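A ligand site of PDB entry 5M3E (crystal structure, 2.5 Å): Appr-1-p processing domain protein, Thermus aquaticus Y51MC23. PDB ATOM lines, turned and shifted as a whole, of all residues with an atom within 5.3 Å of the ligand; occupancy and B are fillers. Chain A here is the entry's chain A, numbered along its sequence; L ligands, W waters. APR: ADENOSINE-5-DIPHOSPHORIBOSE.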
ATOM      1  N   GLY A  17     -21.234  39.621   4.850  1.00  0.00           N
ATOM      2  CA  GLY A  17     -22.483  39.969   4.222  1.00  0.00           C
ATOM      3  C   GLY A  17     -22.662  39.171   2.961  1.00  0.00           C
ATOM      4  O   GLY A  17     -22.097  38.091   2.792  1.00  0.00           O
ATOM      5  N   ASN A  18     -23.476  39.734   2.063  1.00  0.00           N
ATOM      6  CA  ASN A  18     -23.868  39.076   0.840  1.00  0.00           C
ATOM      7  C   ASN A  18     -23.199  39.842  -0.294  1.00  0.00           C
ATOM      8  O   ASN A  18     -23.446  41.033  -0.475  1.00  0.00           O
ATOM      9  CB  ASN A  18     -25.395  39.075   0.725  1.00  0.00           C
ATOM     10  CG  ASN A  18     -25.873  38.821  -0.696  1.00  0.00           C
ATOM     11  OD1 ASN A  18     -25.208  38.168  -1.493  1.00  0.00           O
ATOM     12  ND2 ASN A  18     -27.047  39.326  -1.009  1.00  0.00           N
ATOM     13  N   LEU A  19     -22.355  39.128  -1.047  1.00  0.00           N
ATOM     14  CA  LEU A  19     -21.577  39.661  -2.171  1.00  0.00           C
ATOM     15  C   LEU A  19     -22.430  40.393  -3.211  1.00  0.00           C
ATOM     16  O   LEU A  19     -22.008  41.407  -3.766  1.00  0.00           O
ATOM     17  CB  LEU A  19     -20.837  38.499  -2.862  1.00  0.00           C
ATOM     18  CG  LEU A  19     -20.181  38.741  -4.219  1.00  0.00           C
ATOM     19  CD1 LEU A  19     -19.014  39.683  -4.039  1.00  0.00           C
ATOM     20  CD2 LEU A  19     -19.664  37.432  -4.774  1.00  0.00           C
ATOM     21  N   LEU A  20     -23.602  39.844  -3.502  1.00  0.00           N
ATOM     22  CA  LEU A  20     -24.410  40.262  -4.676  1.00  0.00           C
ATOM     23  C   LEU A  20     -25.065  41.654  -4.540  1.00  0.00           C
ATOM     24  O   LEU A  20     -25.553  42.200  -5.544  1.00  0.00           O
ATOM     25  CB  LEU A  20     -25.510  39.214  -5.002  1.00  0.00           C
ATOM     26  CG  LEU A  20     -25.033  37.945  -5.709  1.00  0.00           C
ATOM     27  CD1 LEU A  20     -24.517  36.891  -4.734  1.00  0.00           C
ATOM     28  CD2 LEU A  20     -26.180  37.381  -6.534  1.00  0.00           C
ATOM     29  N   THR A  30     -17.859  32.585  -8.981  1.00  0.00           N
ATOM     30  CA  THR A  30     -17.068  31.346  -8.982  1.00  0.00           C
ATOM     31  C   THR A  30     -17.761  30.315  -9.871  1.00  0.00           C
ATOM     32  O   THR A  30     -18.859  29.843  -9.534  1.00  0.00           O
ATOM     33  CB  THR A  30     -16.966  30.739  -7.577  1.00  0.00           C
ATOM     34  OG1 THR A  30     -18.274  30.376  -7.101  1.00  0.00           O
ATOM     35  CG2 THR A  30     -16.397  31.732  -6.628  1.00  0.00           C
ATOM     36  N   VAL A  31     -17.106  29.928 -10.955  1.00  0.00           N
ATOM     37  CA  VAL A  31     -17.696  28.990 -11.891  1.00  0.00           C
ATOM     38  C   VAL A  31     -16.820  27.776 -12.155  1.00  0.00           C
ATOM     39  O   VAL A  31     -15.629  27.787 -11.873  1.00  0.00           O
ATOM     40  CB  VAL A  31     -18.085  29.661 -13.241  1.00  0.00           C
ATOM     41  CG1 VAL A  31     -19.065  30.788 -13.015  1.00  0.00           C
ATOM     42  CG2 VAL A  31     -16.865  30.167 -14.023  1.00  0.00           C
ATOM     43  N   ASN A  32     -17.463  26.759 -12.729  1.00  0.00           N
ATOM     44  CA  ASN A  32     -16.769  25.626 -13.326  1.00  0.00           C
ATOM     45  C   ASN A  32     -16.751  25.772 -14.860  1.00  0.00           C
ATOM     46  O   ASN A  32     -17.327  26.702 -15.423  1.00  0.00           O
ATOM     47  CB  ASN A  32     -17.402  24.303 -12.881  1.00  0.00           C
ATOM     48  CG  ASN A  32     -18.829  24.152 -13.335  1.00  0.00           C
ATOM     49  OD1 ASN A  32     -19.099  24.026 -14.530  1.00  0.00           O
ATOM     50  ND2 ASN A  32     -19.782  24.219 -12.359  1.00  0.00           N
ATOM     51  N   VAL A  36     -22.701  24.497 -15.983  1.00  0.00           N
ATOM     52  CA  VAL A  36     -23.765  24.508 -14.993  1.00  0.00           C
ATOM     53  C   VAL A  36     -23.319  25.381 -13.814  1.00  0.00           C
ATOM     54  O   VAL A  36     -22.125  25.451 -13.446  1.00  0.00           O
ATOM     55  CB  VAL A  36     -24.163  23.091 -14.509  1.00  0.00           C
ATOM     56  CG1 VAL A  36     -24.599  22.208 -15.678  1.00  0.00           C
ATOM     57  CG2 VAL A  36     -23.052  22.387 -13.745  1.00  0.00           C
ATOM     58  N   MET A  37     -24.302  26.089 -13.269  1.00  0.00           N
ATOM     59  CA  MET A  37     -24.171  26.871 -12.071  1.00  0.00           C
ATOM     60  C   MET A  37     -25.207  26.247 -11.131  1.00  0.00           C
ATOM     61  O   MET A  37     -26.280  26.808 -10.924  1.00  0.00           O
ATOM     62  CB  MET A  37     -24.531  28.339 -12.369  1.00  0.00           C
ATOM     63  CG  MET A  37     -23.611  29.099 -13.288  1.00  0.00           C
ATOM     64  SD  MET A  37     -23.697  30.883 -13.049  1.00  0.00           S
ATOM     65  CE  MET A  37     -22.918  31.402 -14.561  1.00  0.00           C
ATOM     66  N   GLY A  38     -24.893  25.094 -10.556  1.00  0.00           N
ATOM     67  CA  GLY A  38     -25.849  24.295  -9.771  1.00  0.00           C
ATOM     68  C   GLY A  38     -25.881  24.454  -8.260  1.00  0.00           C
ATOM     69  O   GLY A  38     -26.756  23.861  -7.578  1.00  0.00           O
ATOM     70  N   LYS A  39     -24.933  25.201  -7.718  1.00  0.00           N
ATOM     71  CA  LYS A  39     -24.929  25.457  -6.285  1.00  0.00           C
ATOM     72  C   LYS A  39     -23.975  26.563  -5.830  1.00  0.00           C
ATOM     73  O   LYS A  39     -23.251  27.127  -6.642  1.00  0.00           O
ATOM     74  CB  LYS A  39     -24.649  24.148  -5.509  1.00  0.00           C
ATOM     75  CG  LYS A  39     -23.700  23.188  -6.203  1.00  0.00           C
ATOM     76  CD  LYS A  39     -23.062  22.288  -5.173  1.00  0.00           C
ATOM     77  CE  LYS A  39     -22.598  21.003  -5.779  1.00  0.00           C
ATOM     78  NZ  LYS A  39     -22.988  19.901  -4.872  1.00  0.00           N
ATOM     79  N   GLY A  40     -24.042  26.899  -4.533  1.00  0.00           N
ATOM     80  CA  GLY A  40     -23.165  27.870  -3.894  1.00  0.00           C
ATOM     81  C   GLY A  40     -23.422  29.265  -4.427  1.00  0.00           C
ATOM     82  O   GLY A  40     -24.568  29.656  -4.670  1.00  0.00           O
ATOM     83  N   VAL A  41     -22.330  29.995  -4.658  1.00  0.00           N
ATOM     84  CA  VAL A  41     -22.354  31.361  -5.196  1.00  0.00           C
ATOM     85  C   VAL A  41     -22.898  31.377  -6.623  1.00  0.00           C
ATOM     86  O   VAL A  41     -23.572  32.324  -7.035  1.00  0.00           O
ATOM     87  CB  VAL A  41     -20.915  31.946  -5.208  1.00  0.00           C
ATOM     88  CG1 VAL A  41     -20.802  33.229  -6.029  1.00  0.00           C
ATOM     89  CG2 VAL A  41     -20.417  32.163  -3.783  1.00  0.00           C
ATOM     90  N   ALA A  42     -22.568  30.350  -7.392  1.00  0.00           N
ATOM     91  CA  ALA A  42     -22.872  30.355  -8.796  1.00  0.00           C
ATOM     92  C   ALA A  42     -24.377  30.212  -8.974  1.00  0.00           C
ATOM     93  O   ALA A  42     -24.927  30.801  -9.883  1.00  0.00           O
ATOM     94  CB  ALA A  42     -22.113  29.266  -9.534  1.00  0.00           C
ATOM     95  N   LEU A  43     -25.035  29.452  -8.097  1.00  0.00           N
ATOM     96  CA  LEU A  43     -26.493  29.308  -8.141  1.00  0.00           C
ATOM     97  C   LEU A  43     -27.195  30.649  -7.904  1.00  0.00           C
ATOM     98  O   LEU A  43     -28.095  31.005  -8.656  1.00  0.00           O
ATOM     99  CB  LEU A  43     -26.969  28.301  -7.117  1.00  0.00           C
ATOM    100  CG  LEU A  43     -28.467  27.964  -6.997  1.00  0.00           C
ATOM    101  CD1 LEU A  43     -29.055  27.635  -8.365  1.00  0.00           C
ATOM    102  CD2 LEU A  43     -28.637  26.806  -6.042  1.00  0.00           C
ATOM    103  N   GLN A  44     -26.702  31.397  -6.917  1.00  0.00           N
ATOM    104  CA  GLN A  44     -27.234  32.743  -6.606  1.00  0.00           C
ATOM    105  C   GLN A  44     -27.035  33.695  -7.763  1.00  0.00           C
ATOM    106  O   GLN A  44     -27.964  34.457  -8.071  1.00  0.00           O
ATOM    107  CB  GLN A  44     -26.582  33.340  -5.348  1.00  0.00           C
ATOM    108  CG  GLN A  44     -26.790  32.522  -4.072  1.00  0.00           C
ATOM    109  CD  GLN A  44     -25.787  32.861  -2.971  1.00  0.00           C
ATOM    110  OE1 GLN A  44     -25.837  33.951  -2.448  1.00  0.00           O
ATOM    111  NE2 GLN A  44     -24.905  31.916  -2.606  1.00  0.00           N
ATOM    112  N   THR A  89     -12.937  28.585 -10.817  1.00  0.00           N
ATOM    113  CA  THR A  89     -12.336  27.900  -9.683  1.00  0.00           C
ATOM    114  C   THR A  89     -12.437  26.368  -9.752  1.00  0.00           C
ATOM    115  O   THR A  89     -11.900  25.683  -8.878  1.00  0.00           O
ATOM    116  CB  THR A  89     -12.947  28.363  -8.375  1.00  0.00           C
ATOM    117  OG1 THR A  89     -14.249  27.845  -8.278  1.00  0.00           O
ATOM    118  CG2 THR A  89     -12.991  29.888  -8.330  1.00  0.00           C
ATOM    119  N   LYS A  90     -13.114  25.842 -10.775  1.00  0.00           N
ATOM    120  CA  LYS A  90     -13.134  24.403 -11.029  1.00  0.00           C
ATOM    121  C   LYS A  90     -13.073  24.107 -12.512  1.00  0.00           C
ATOM    122  O   LYS A  90     -13.449  24.948 -13.318  1.00  0.00           O
ATOM    123  CB  LYS A  90     -14.411  23.769 -10.460  1.00  0.00           C
ATOM    124  CG  LYS A  90     -14.364  23.537  -8.968  1.00  0.00           C
ATOM    125  CD  LYS A  90     -15.548  22.732  -8.504  1.00  0.00           C
ATOM    126  CE  LYS A  90     -15.447  22.434  -7.018  1.00  0.00           C
ATOM    127  NZ  LYS A  90     -16.344  21.291  -6.658  1.00  0.00           N
ATOM    128  N   TRP A  93     -17.294  20.064 -12.047  1.00  0.00           N
ATOM    129  CA  TRP A  93     -17.920  20.257 -10.724  1.00  0.00           C
ATOM    130  C   TRP A  93     -17.702  19.101  -9.707  1.00  0.00           C
ATOM    131  O   TRP A  93     -17.831  19.292  -8.510  1.00  0.00           O
ATOM    132  CB  TRP A  93     -19.432  20.533 -10.885  1.00  0.00           C
ATOM    133  CG  TRP A  93     -20.183  19.438 -11.637  1.00  0.00           C
ATOM    134  CD1 TRP A  93     -20.557  19.472 -12.942  1.00  0.00           C
ATOM    135  CD2 TRP A  93     -20.616  18.177 -11.123  1.00  0.00           C
ATOM    136  NE1 TRP A  93     -21.192  18.310 -13.288  1.00  0.00           N
ATOM    137  CE2 TRP A  93     -21.243  17.492 -12.184  1.00  0.00           C
ATOM    138  CE3 TRP A  93     -20.544  17.537  -9.869  1.00  0.00           C
ATOM    139  CZ2 TRP A  93     -21.791  16.200 -12.032  1.00  0.00           C
ATOM    140  CZ3 TRP A  93     -21.060  16.259  -9.725  1.00  0.00           C
ATOM    141  CH2 TRP A  93     -21.683  15.610 -10.795  1.00  0.00           C
ATOM    142  N   PRO A 124     -15.921  36.697  -3.564  1.00  0.00           N
ATOM    143  CA  PRO A 124     -16.103  35.739  -2.502  1.00  0.00           C
ATOM    144  C   PRO A 124     -14.792  34.985  -2.209  1.00  0.00           C
ATOM    145  O   PRO A 124     -13.770  35.298  -2.853  1.00  0.00           O
ATOM    146  CB  PRO A 124     -17.144  34.803  -3.091  1.00  0.00           C
ATOM    147  CG  PRO A 124     -16.766  34.739  -4.533  1.00  0.00           C
ATOM    148  CD  PRO A 124     -16.181  36.086  -4.874  1.00  0.00           C
ATOM    149  N   PRO A 125     -14.819  33.990  -1.256  1.00  0.00           N
ATOM    150  CA  PRO A 125     -13.691  33.089  -1.012  1.00  0.00           C
ATOM    151  C   PRO A 125     -13.564  32.037  -2.124  1.00  0.00           C
ATOM    152  O   PRO A 125     -14.195  30.964  -2.066  1.00  0.00           O
ATOM    153  CB  PRO A 125     -14.016  32.456   0.367  1.00  0.00           C
ATOM    154  CG  PRO A 125     -14.990  33.400   0.994  1.00  0.00           C
ATOM    155  CD  PRO A 125     -15.831  33.828  -0.188  1.00  0.00           C
ATOM    156  N   LEU A 126     -12.697  32.380  -3.076  1.00  0.00           N
ATOM    157  CA  LEU A 126     -12.476  31.619  -4.304  1.00  0.00           C
ATOM    158  C   LEU A 126     -11.938  30.222  -3.973  1.00  0.00           C
ATOM    159  O   LEU A 126     -10.904  30.096  -3.335  1.00  0.00           O
ATOM    160  CB  LEU A 126     -11.489  32.371  -5.217  1.00  0.00           C
ATOM    161  CG  LEU A 126     -11.625  33.899  -5.395  1.00  0.00           C
ATOM    162  CD1 LEU A 126     -10.449  34.482  -6.209  1.00  0.00           C
ATOM    163  CD2 LEU A 126     -12.945  34.277  -6.034  1.00  0.00           C
ATOM    164  N   GLY A 127     -12.666  29.192  -4.380  1.00  0.00           N
ATOM    165  CA  GLY A 127     -12.260  27.805  -4.173  1.00  0.00           C
ATOM    166  C   GLY A 127     -12.485  27.210  -2.795  1.00  0.00           C
ATOM    167  O   GLY A 127     -12.255  26.001  -2.614  1.00  0.00           O
ATOM    168  N   ALA A 128     -12.944  28.004  -1.835  1.00  0.00           N
ATOM    169  CA  ALA A 128     -12.958  27.591  -0.421  1.00  0.00           C
ATOM    170  C   ALA A 128     -14.287  27.031   0.114  1.00  0.00           C
ATOM    171  O   ALA A 128     -14.375  26.697   1.290  1.00  0.00           O
ATOM    172  CB  ALA A 128     -12.441  28.744   0.455  1.00  0.00           C
ATOM    173  N   GLY A 129     -15.285  26.882  -0.748  1.00  0.00           N
ATOM    174  CA  GLY A 129     -16.525  26.234  -0.402  1.00  0.00           C
ATOM    175  C   GLY A 129     -16.551  24.865  -1.030  1.00  0.00           C
ATOM    176  O   GLY A 129     -15.871  23.941  -0.565  1.00  0.00           O
ATOM    177  N   ASN A 130     -17.303  24.737  -2.107  1.00  0.00           N
ATOM    178  CA  ASN A 130     -17.352  23.468  -2.839  1.00  0.00           C
ATOM    179  C   ASN A 130     -16.008  23.036  -3.458  1.00  0.00           C
ATOM    180  O   ASN A 130     -15.834  21.875  -3.793  1.00  0.00           O
ATOM    181  CB  ASN A 130     -18.443  23.536  -3.908  1.00  0.00           C
ATOM    182  CG  ASN A 130     -19.828  23.775  -3.321  1.00  0.00           C
ATOM    183  OD1 ASN A 130     -20.211  23.145  -2.308  1.00  0.00           O
ATOM    184  ND2 ASN A 130     -20.577  24.703  -3.925  1.00  0.00           N
ATOM    185  N   GLY A 131     -15.072  23.982  -3.599  1.00  0.00           N
ATOM    186  CA  GLY A 131     -13.709  23.697  -4.011  1.00  0.00           C
ATOM    187  C   GLY A 131     -12.778  23.083  -2.974  1.00  0.00           C
ATOM    188  O   GLY A 131     -11.767  22.496  -3.372  1.00  0.00           O
ATOM    189  N   GLY A 132     -13.078  23.218  -1.671  1.00  0.00           N
ATOM    190  CA  GLY A 132     -12.326  22.562  -0.603  1.00  0.00           C
ATOM    191  C   GLY A 132     -10.951  23.142  -0.253  1.00  0.00           C
ATOM    192  O   GLY A 132     -10.218  22.550   0.535  1.00  0.00           O
ATOM    193  N   TYR A 157     -15.310  39.123   0.546  1.00  0.00           N
ATOM    194  CA  TYR A 157     -16.283  38.608   1.498  1.00  0.00           C
ATOM    195  C   TYR A 157     -15.730  37.370   2.181  1.00  0.00           C
ATOM    196  O   TYR A 157     -15.746  36.304   1.581  1.00  0.00           O
ATOM    197  CB  TYR A 157     -17.636  38.328   0.815  1.00  0.00           C
ATOM    198  CG  TYR A 157     -18.369  39.613   0.554  1.00  0.00           C
ATOM    199  CD1 TYR A 157     -17.946  40.477  -0.457  1.00  0.00           C
ATOM    200  CD2 TYR A 157     -19.443  40.009   1.362  1.00  0.00           C
ATOM    201  CE1 TYR A 157     -18.592  41.676  -0.677  1.00  0.00           C
ATOM    202  CE2 TYR A 157     -20.093  41.218   1.144  1.00  0.00           C
ATOM    203  CZ  TYR A 157     -19.664  42.042   0.122  1.00  0.00           C
ATOM    204  OH  TYR A 157     -20.278  43.251  -0.130  1.00  0.00           O
ATOM    205  N   PRO A 159     -15.546  34.145   4.657  1.00  0.00           N
ATOM    206  CA  PRO A 159     -16.625  33.231   5.050  1.00  0.00           C
ATOM    207  C   PRO A 159     -16.872  33.184   6.582  1.00  0.00           C
ATOM    208  O   PRO A 159     -16.302  33.993   7.327  1.00  0.00           O
ATOM    209  CB  PRO A 159     -16.123  31.886   4.533  1.00  0.00           C
ATOM    210  CG  PRO A 159     -14.641  31.982   4.634  1.00  0.00           C
ATOM    211  CD  PRO A 159     -14.267  33.422   4.502  1.00  0.00           C
ATOM    212  N   VAL A 160     -17.748  32.271   7.025  1.00  0.00           N
ATOM    213  CA  VAL A 160     -17.729  31.746   8.411  1.00  0.00           C
ATOM    214  C   VAL A 160     -18.475  30.407   8.532  1.00  0.00           C
ATOM    215  O   VAL A 160     -18.972  29.864   7.546  1.00  0.00           O
ATOM    216  CB  VAL A 160     -18.262  32.762   9.477  1.00  0.00           C
ATOM    217  CG1 VAL A 160     -19.780  32.935   9.378  1.00  0.00           C
ATOM    218  CG2 VAL A 160     -17.852  32.328  10.878  1.00  0.00           C
HETATM  219  N1  APR L   1     -21.875  36.388  -0.468  1.00  0.00           N
HETATM  220  C2  APR L   1     -20.621  36.164  -0.005  1.00  0.00           C
HETATM  221  N3  APR L   1     -20.115  34.931   0.174  1.00  0.00           N
HETATM  222  C4  APR L   1     -20.864  33.830  -0.098  1.00  0.00           C
HETATM  223  C5  APR L   1     -22.245  33.983  -0.612  1.00  0.00           C
HETATM  224  C6  APR L   1     -22.715  35.381  -0.779  1.00  0.00           C
HETATM  225  N6  APR L   1     -23.953  35.651  -1.233  1.00  0.00           N
HETATM  226  N7  APR L   1     -22.741  32.742  -0.800  1.00  0.00           N
HETATM  227  C8  APR L   1     -21.760  31.860  -0.451  1.00  0.00           C
HETATM  228  N9  APR L   1     -20.646  32.530  -0.017  1.00  0.00           N
HETATM  229  C1' APR L   1     -19.341  31.982   0.420  1.00  0.00           C
HETATM  230  C2' APR L   1     -19.420  30.672   1.176  1.00  0.00           C
HETATM  231  O2' APR L   1     -18.564  30.771   2.318  1.00  0.00           O
HETATM  232  C3' APR L   1     -18.857  29.638   0.244  1.00  0.00           C
HETATM  233  O3' APR L   1     -18.172  28.578   0.939  1.00  0.00           O
HETATM  234  O4' APR L   1     -18.578  31.747  -0.767  1.00  0.00           O
HETATM  235  C4' APR L   1     -17.938  30.479  -0.648  1.00  0.00           C
HETATM  236  C5' APR L   1     -17.638  29.938  -2.042  1.00  0.00           C
HETATM  237  O5' APR L   1     -18.831  29.482  -2.691  1.00  0.00           O
HETATM  238  PA  APR L   1     -18.751  28.225  -3.699  1.00  0.00           P
HETATM  239  O1A APR L   1     -19.939  28.376  -4.616  1.00  0.00           O
HETATM  240  O2A APR L   1     -18.561  26.964  -2.901  1.00  0.00           O
HETATM  241  O3A APR L   1     -17.430  28.563  -4.584  1.00  0.00           O
HETATM  242  PB  APR L   1     -16.192  27.554  -4.901  1.00  0.00           P
HETATM  243  O1B APR L   1     -15.713  26.932  -3.619  1.00  0.00           O
HETATM  244  O2B APR L   1     -15.176  28.289  -5.789  1.00  0.00           O
HETATM  245  O5D APR L   1     -16.804  26.381  -5.803  1.00  0.00           O
HETATM  246  C5D APR L   1     -17.022  26.455  -7.223  1.00  0.00           C
HETATM  247  O4D APR L   1     -19.333  25.800  -6.815  1.00  0.00           O
HETATM  248  O1D APR L   1     -20.295  27.898  -7.049  1.00  0.00           O
HETATM  249  C1D APR L   1     -20.236  26.575  -7.592  1.00  0.00           C
HETATM  250  O2D APR L   1     -20.759  26.359  -9.966  1.00  0.00           O
HETATM  251  C2D APR L   1     -19.715  26.617  -9.022  1.00  0.00           C
HETATM  252  O3D APR L   1     -18.958  24.359  -9.614  1.00  0.00           O
HETATM  253  C3D APR L   1     -18.567  25.623  -9.066  1.00  0.00           C
HETATM  254  C4D APR L   1     -18.165  25.499  -7.596  1.00  0.00           C
HETATM  255  O   HOH W   1     -20.272  27.239 -12.584  1.00  0.00           O
HETATM  256  O   HOH W   2     -20.811  26.600  -1.173  1.00  0.00           O
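Water W1 lies within hydrogen-bond range of the backbone carbonyl oxygen of Val 36 (2.7 Å), an oxygen (O2D) of the ligand (2.8 Å) and the backbone NH of Asn 32 (2.9 Å).
Water W2 bridges O2A of the ligand and ND2 of Asn 130.
Merely in contact with the ligand: Gly 17, Leu 20, Val 36, Gly 40, Lys 90, Pro 125, Tyr 157 and Pro 159.
Within 4 Å of the ligand: Gly 17, Asn 18, Leu 19, Leu 20, Thr 30, Asn 32, Val 36, Lys 39, Gly 40, Val 41, Ala 42, Gln 44, Thr 89, Lys 90, Pro 125, Gly 127, Ala 128, Gly 129, Asn 130, Gly 131, Tyr 157 and Pro 159.
O of Asn 130 lies within hydrogen-bond range of NZ of Lys 90 (3.0 Å).
The backbone NH of Thr 89 lies within hydrogen-bond range of the backbone carbonyl oxygen of Val 31 (3.0 Å).
The backbone carbonyl oxygen of Gly 40 sits at hydrogen-bond distance from the side-chain amide nitrogen of Gln 44 (3.1 Å).
The backbone NH of Leu 20 lies within hydrogen-bond range of the side-chain amide oxygen of Asn 18 (3.1 Å).
The side-chain amide nitrogen of Asn 32 is in hydrogen-bond range of the backbone carbonyl oxygen of Val 36.
O of Gly 127 is in hydrogen-bond range of N of Gly 132 (3.1 Å).
The side-chain amino group (NZ) of Lys 90 sits at hydrogen-bond distance from the backbone carbonyl oxygen (O) of Trp 93.
The backbone NH of Lys 90 sits at hydrogen-bond distance from the backbone carbonyl oxygen of Val 31, at 3.4 Å.
An oxygen (O2A) of the ligand sits at hydrogen-bond distance from the backbone NH (N) of Asn 130, at 2.7 Å.
O2A of the ligand is in hydrogen-bond range of ND2 of Asn 130 (3.2 Å).
OG1 of Thr 89 sits at hydrogen-bond distance from O2B of the ligand (2.7 Å).
OE1 of Gln 44 sits at hydrogen-bond distance from N6 of the ligand (2.8 Å).
OD1 of Asn 18 lies within hydrogen-bond range of N6 of the ligand (2.8 Å).
The backbone NH (N) of Leu 19 is in hydrogen-bond range of a nitrogen (N1) of the ligand, at 2.8 Å.
O3D of the ligand lies within hydrogen-bond range of ND2 of Asn 32 (2.9 Å).
O1A of the ligand is in hydrogen-bond range of N of Val 41, 2.9 Å away.
N of Gly 129 sits at hydrogen-bond distance from O1B of the ligand (2.9 Å).
An oxygen (O2B) of the ligand sits at hydrogen-bond distance from the backbone NH (N) of Gly 127.
N of Gly 131 lies within hydrogen-bond range of O1B of the ligand (3.0 Å).
An oxygen (O1D) of the ligand is in hydrogen-bond range of the backbone carbonyl oxygen of Lys 39, at 3.1 Å.
An oxygen (O1D) of the ligand sits close to the backbone carbonyl oxygen (O) of Thr 30 (3.5 Å).
The side-chain hydroxyl (OG1) of Thr 30 sits at hydrogen-bond distance from an oxygen (O1D) of the ligand, 3.2 Å away.
The backbone NH (N) of Ala 42 sits at hydrogen-bond distance from an oxygen (O1D) of the ligand (3.4 Å).
An oxygen (O1B) of the ligand sits at hydrogen-bond distance from the backbone NH of Ala 128, at 3.5 Å.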
